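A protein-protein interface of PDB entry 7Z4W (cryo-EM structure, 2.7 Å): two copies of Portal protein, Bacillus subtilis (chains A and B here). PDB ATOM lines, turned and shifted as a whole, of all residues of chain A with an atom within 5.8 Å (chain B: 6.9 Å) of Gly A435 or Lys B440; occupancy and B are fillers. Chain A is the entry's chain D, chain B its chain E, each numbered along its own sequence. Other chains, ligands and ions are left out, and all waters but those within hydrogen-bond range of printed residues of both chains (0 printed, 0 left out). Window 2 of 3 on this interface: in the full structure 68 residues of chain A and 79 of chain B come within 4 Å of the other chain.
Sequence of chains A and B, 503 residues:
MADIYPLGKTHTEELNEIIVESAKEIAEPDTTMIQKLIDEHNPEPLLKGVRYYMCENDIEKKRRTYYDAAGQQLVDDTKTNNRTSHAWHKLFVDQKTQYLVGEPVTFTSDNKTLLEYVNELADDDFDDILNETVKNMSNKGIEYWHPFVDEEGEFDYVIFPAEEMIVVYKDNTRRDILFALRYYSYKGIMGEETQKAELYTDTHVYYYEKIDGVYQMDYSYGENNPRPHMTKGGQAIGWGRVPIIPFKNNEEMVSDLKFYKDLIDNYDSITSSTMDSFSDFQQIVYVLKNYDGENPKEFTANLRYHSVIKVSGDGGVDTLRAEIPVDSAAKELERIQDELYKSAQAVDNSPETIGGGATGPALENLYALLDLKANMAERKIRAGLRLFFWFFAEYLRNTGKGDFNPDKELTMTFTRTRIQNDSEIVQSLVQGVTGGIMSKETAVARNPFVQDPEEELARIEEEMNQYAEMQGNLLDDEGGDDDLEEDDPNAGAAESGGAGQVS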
ATOM      1  N   VAL A 430      -3.984  11.227   1.010  1.00  0.00           N
ATOM      2  CA  VAL A 430      -4.687  12.085   1.961  1.00  0.00           C
ATOM      3  C   VAL A 430      -4.419  11.630   3.392  1.00  0.00           C
ATOM      4  O   VAL A 430      -4.179  12.458   4.285  1.00  0.00           O
ATOM      5  CB  VAL A 430      -6.192  12.120   1.621  1.00  0.00           C
ATOM      6  CG1 VAL A 430      -7.023  12.634   2.782  1.00  0.00           C
ATOM      7  CG2 VAL A 430      -6.427  12.991   0.406  1.00  0.00           C
ATOM      8  N   GLN A 431      -4.385  10.309   3.615  1.00  0.00           N
ATOM      9  CA  GLN A 431      -4.060   9.779   4.937  1.00  0.00           C
ATOM     10  C   GLN A 431      -2.627  10.115   5.352  1.00  0.00           C
ATOM     11  O   GLN A 431      -2.374  10.454   6.515  1.00  0.00           O
ATOM     12  CB  GLN A 431      -4.283   8.273   4.948  1.00  0.00           C
ATOM     13  CG  GLN A 431      -4.310   7.660   6.313  1.00  0.00           C
ATOM     14  CD  GLN A 431      -4.761   6.221   6.271  1.00  0.00           C
ATOM     15  OE1 GLN A 431      -5.051   5.684   5.201  1.00  0.00           O
ATOM     16  NE2 GLN A 431      -4.838   5.591   7.435  1.00  0.00           N
ATOM     17  N   GLY A 432      -1.683  10.059   4.409  1.00  0.00           N
ATOM     18  CA  GLY A 432      -0.308  10.410   4.721  1.00  0.00           C
ATOM     19  C   GLY A 432      -0.082  11.889   4.986  1.00  0.00           C
ATOM     20  O   GLY A 432       0.761  12.246   5.812  1.00  0.00           O
ATOM     21  N   VAL A 433      -0.809  12.765   4.288  1.00  0.00           N
ATOM     22  CA  VAL A 433      -0.686  14.199   4.547  1.00  0.00           C
ATOM     23  C   VAL A 433      -1.321  14.563   5.887  1.00  0.00           C
ATOM     24  O   VAL A 433      -0.763  15.356   6.656  1.00  0.00           O
ATOM     25  CB  VAL A 433      -1.286  15.005   3.377  1.00  0.00           C
ATOM     26  CG1 VAL A 433      -1.408  16.476   3.709  1.00  0.00           C
ATOM     27  CG2 VAL A 433      -0.409  14.868   2.175  1.00  0.00           C
ATOM     28  N   THR A 434      -2.476  13.968   6.204  1.00  0.00           N
ATOM     29  CA  THR A 434      -3.118  14.229   7.490  1.00  0.00           C
ATOM     30  C   THR A 434      -2.302  13.671   8.657  1.00  0.00           C
ATOM     31  O   THR A 434      -2.231  14.301   9.718  1.00  0.00           O
ATOM     32  CB  THR A 434      -4.537  13.654   7.471  1.00  0.00           C
ATOM     33  OG1 THR A 434      -5.264  14.239   6.387  1.00  0.00           O
ATOM     34  CG2 THR A 434      -5.284  13.943   8.758  1.00  0.00           C
ATOM     35  N   GLY A 435      -1.628  12.535   8.465  1.00  0.00           N
ATOM     36  CA  GLY A 435      -0.791  11.980   9.516  1.00  0.00           C
ATOM     37  C   GLY A 435       0.493  12.741   9.781  1.00  0.00           C
ATOM     38  O   GLY A 435       1.099  12.557  10.840  1.00  0.00           O
ATOM     39  N   GLY A 436       0.927  13.583   8.850  1.00  0.00           N
ATOM     40  CA  GLY A 436       2.117  14.382   9.044  1.00  0.00           C
ATOM     41  C   GLY A 436       3.414  13.776   8.556  1.00  0.00           C
ATOM     42  O   GLY A 436       4.479  14.329   8.844  1.00  0.00           O
ATOM     43  N   ILE A 437       3.369  12.666   7.828  1.00  0.00           N
ATOM     44  CA  ILE A 437       4.575  12.000   7.359  1.00  0.00           C
ATOM     45  C   ILE A 437       4.875  12.341   5.897  1.00  0.00           C
ATOM     46  O   ILE A 437       5.678  11.668   5.258  1.00  0.00           O
ATOM     47  CB  ILE A 437       4.495  10.480   7.570  1.00  0.00           C
ATOM     48  CG1 ILE A 437       3.360   9.872   6.744  1.00  0.00           C
ATOM     49  CG2 ILE A 437       4.301  10.162   9.036  1.00  0.00           C
ATOM     50  CD1 ILE A 437       3.380   8.367   6.698  1.00  0.00           C
ATOM     51  N   VAL B 430       1.219   5.671  10.023  1.00  0.00           N
ATOM     52  CA  VAL B 430       0.426   6.722  10.656  1.00  0.00           C
ATOM     53  C   VAL B 430      -0.059   6.276  12.034  1.00  0.00           C
ATOM     54  O   VAL B 430      -0.017   7.048  13.003  1.00  0.00           O
ATOM     55  CB  VAL B 430      -0.734   7.125   9.722  1.00  0.00           C
ATOM     56  CG1 VAL B 430      -1.843   7.847  10.465  1.00  0.00           C
ATOM     57  CG2 VAL B 430      -0.212   7.985   8.590  1.00  0.00           C
ATOM     58  N   VAL B 433       2.962   6.402  14.447  1.00  0.00           N
ATOM     59  CA  VAL B 433       3.325   7.764  14.832  1.00  0.00           C
ATOM     60  C   VAL B 433       2.307   8.332  15.816  1.00  0.00           C
ATOM     61  O   VAL B 433       2.675   8.949  16.824  1.00  0.00           O
ATOM     62  CB  VAL B 433       3.485   8.640  13.574  1.00  0.00           C
ATOM     63  CG1 VAL B 433       3.280  10.115  13.871  1.00  0.00           C
ATOM     64  CG2 VAL B 433       4.855   8.433  12.978  1.00  0.00           C
ATOM     65  N   THR B 434       1.016   8.094  15.567  1.00  0.00           N
ATOM     66  CA  THR B 434      -0.032   8.576  16.463  1.00  0.00           C
ATOM     67  C   THR B 434       0.008   7.866  17.814  1.00  0.00           C
ATOM     68  O   THR B 434      -0.273   8.485  18.847  1.00  0.00           O
ATOM     69  CB  THR B 434      -1.391   8.399  15.782  1.00  0.00           C
ATOM     70  OG1 THR B 434      -1.352   9.024  14.495  1.00  0.00           O
ATOM     71  CG2 THR B 434      -2.508   9.038  16.580  1.00  0.00           C
ATOM     72  N   MET B 438       7.038   5.745  17.645  1.00  0.00           N
ATOM     73  CA  MET B 438       7.816   5.946  16.434  1.00  0.00           C
ATOM     74  C   MET B 438       8.052   7.433  16.231  1.00  0.00           C
ATOM     75  O   MET B 438       7.161   8.245  16.480  1.00  0.00           O
ATOM     76  CB  MET B 438       7.097   5.356  15.217  1.00  0.00           C
ATOM     77  CG  MET B 438       7.967   5.211  14.013  1.00  0.00           C
ATOM     78  SD  MET B 438       7.178   4.379  12.636  1.00  0.00           S
ATOM     79  CE  MET B 438       8.598   4.233  11.564  1.00  0.00           C
ATOM     80  N   SER B 439       9.250   7.778  15.773  1.00  0.00           N
ATOM     81  CA  SER B 439       9.560   9.150  15.409  1.00  0.00           C
ATOM     82  C   SER B 439       8.969   9.493  14.049  1.00  0.00           C
ATOM     83  O   SER B 439       8.735   8.622  13.208  1.00  0.00           O
ATOM     84  CB  SER B 439      11.070   9.369  15.385  1.00  0.00           C
ATOM     85  OG  SER B 439      11.387  10.676  14.961  1.00  0.00           O
ATOM     86  N   LYS B 440       8.729  10.787  13.840  1.00  0.00           N
ATOM     87  CA  LYS B 440       8.217  11.262  12.561  1.00  0.00           C
ATOM     88  C   LYS B 440       9.272  11.175  11.464  1.00  0.00           C
ATOM     89  O   LYS B 440       8.935  10.911  10.305  1.00  0.00           O
ATOM     90  CB  LYS B 440       7.717  12.696  12.715  1.00  0.00           C
ATOM     91  CG  LYS B 440       6.703  13.133  11.693  1.00  0.00           C
ATOM     92  CD  LYS B 440       6.163  14.510  12.028  1.00  0.00           C
ATOM     93  CE  LYS B 440       5.209  14.464  13.211  1.00  0.00           C
ATOM     94  NZ  LYS B 440       4.026  13.612  12.927  1.00  0.00           N
ATOM     95  N   GLU B 441      10.546  11.368  11.818  1.00  0.00           N
ATOM     96  CA  GLU B 441      11.636  11.316  10.847  1.00  0.00           C
ATOM     97  C   GLU B 441      11.831   9.908  10.293  1.00  0.00           C
ATOM     98  O   GLU B 441      12.038   9.729   9.083  1.00  0.00           O
ATOM     99  CB  GLU B 441      12.920  11.826  11.503  1.00  0.00           C
ATOM    100  CG  GLU B 441      14.155  11.753  10.634  1.00  0.00           C
ATOM    101  CD  GLU B 441      15.394  12.279  11.328  1.00  0.00           C
ATOM    102  OE1 GLU B 441      15.306  12.637  12.520  1.00  0.00           O
ATOM    103  OE2 GLU B 441      16.460  12.338  10.682  1.00  0.00           O
ATOM    104  N   THR B 442      11.744   8.897  11.162  1.00  0.00           N
ATOM    105  CA  THR B 442      11.842   7.509  10.723  1.00  0.00           C
ATOM    106  C   THR B 442      10.668   7.127   9.831  1.00  0.00           C
ATOM    107  O   THR B 442      10.840   6.395   8.855  1.00  0.00           O
ATOM    108  CB  THR B 442      11.919   6.580  11.936  1.00  0.00           C
ATOM    109  OG1 THR B 442      12.907   7.068  12.851  1.00  0.00           O
ATOM    110  CG2 THR B 442      12.296   5.167  11.522  1.00  0.00           C
ATOM    111  N   ALA B 443       9.474   7.643  10.129  1.00  0.00           N
ATOM    112  CA  ALA B 443       8.311   7.325   9.310  1.00  0.00           C
ATOM    113  C   ALA B 443       8.350   8.037   7.965  1.00  0.00           C
ATOM    114  O   ALA B 443       7.799   7.526   6.986  1.00  0.00           O
ATOM    115  CB  ALA B 443       7.028   7.678  10.056  1.00  0.00           C
ATOM    116  N   VAL B 444       8.980   9.213   7.896  1.00  0.00           N
ATOM    117  CA  VAL B 444       9.223   9.836   6.599  1.00  0.00           C
ATOM    118  C   VAL B 444      10.227   9.010   5.800  1.00  0.00           C
ATOM    119  O   VAL B 444      10.082   8.834   4.585  1.00  0.00           O
ATOM    120  CB  VAL B 444       9.674  11.299   6.785  1.00  0.00           C
ATOM    121  CG1 VAL B 444      10.185  11.905   5.491  1.00  0.00           C
ATOM    122  CG2 VAL B 444       8.530  12.139   7.304  1.00  0.00           C
ATOM    123  N   ALA B 445      11.219   8.429   6.477  1.00  0.00           N
ATOM    124  CA  ALA B 445      12.197   7.606   5.773  1.00  0.00           C
ATOM    125  C   ALA B 445      11.662   6.247   5.312  1.00  0.00           C
ATOM    126  O   ALA B 445      12.346   5.581   4.534  1.00  0.00           O
ATOM    127  CB  ALA B 445      13.428   7.397   6.651  1.00  0.00           C
ATOM    128  N   LEU B 457      11.817  16.409   4.762  1.00  0.00           N
ATOM    129  CA  LEU B 457      11.730  16.975   6.106  1.00  0.00           C
ATOM    130  C   LEU B 457      11.863  18.492   6.084  1.00  0.00           C
ATOM    131  O   LEU B 457      11.148  19.194   6.815  1.00  0.00           O
ATOM    132  CB  LEU B 457      12.802  16.365   7.003  1.00  0.00           C
ATOM    133  CG  LEU B 457      12.580  14.922   7.442  1.00  0.00           C
ATOM    134  CD1 LEU B 457      13.891  14.300   7.868  1.00  0.00           C
ATOM    135  CD2 LEU B 457      11.549  14.854   8.554  1.00  0.00           C
ATOM    136  N   ILE B 460       8.481  19.832   4.885  1.00  0.00           N
ATOM    137  CA  ILE B 460       7.456  19.839   5.930  1.00  0.00           C
ATOM    138  C   ILE B 460       7.725  20.959   6.936  1.00  0.00           C
ATOM    139  O   ILE B 460       6.793  21.636   7.397  1.00  0.00           O
ATOM    140  CB  ILE B 460       7.372  18.455   6.604  1.00  0.00           C
ATOM    141  CG1 ILE B 460       6.934  17.395   5.596  1.00  0.00           C
ATOM    142  CG2 ILE B 460       6.400  18.452   7.759  1.00  0.00           C
ATOM    143  CD1 ILE B 460       6.915  15.989   6.142  1.00  0.00           C
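The backbone NH (N) of Ile A437 lies within hydrogen-bond range of the backbone carbonyl oxygen (O) of Gly A432 (3.3 Å). The backbone carbonyl oxygen of Val B430 sits at hydrogen-bond distance from the side-chain hydroxyl of Thr B434.
Among the printed residues, pairs that only touch across the chains: Gln A431 with Val B430, Gly A435 with Lys B440, Gly A436 with Lys B440, Gly A436 with Ile B460, Ile A437 with Ala B443 and Ile A437 with Val B444.
Of the printed residues of chain B, Gly A435 touches Lys B440. Lys B440 touches just these residues of chain A: Gly A435 and Gly A436. Printed residues of chain A within 4 Å of Ala B443: Ile A437. Of the printed residues of chain A, Val B444 touches Ile A437. Of the printed residues of chain A, Ile B460 touches Gly A436 (3.999 Å). Of the printed residues of chain B, Gly A436 touches Lys B440 and Ile B460. Printed residues of chain A within 4 Å of Val B430: Gln A431. The nearest printed residue of chain B that does not touch Ile A437 is Val B430 (4.1 Å).
Of the 8 printed residues of chain A, 4 touch a printed residue of chain B.
3 positions are printed for both chains. Of the 6 pairs that touch across the chains among the printed residues, none has its exchanged pair printed and touching as well.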
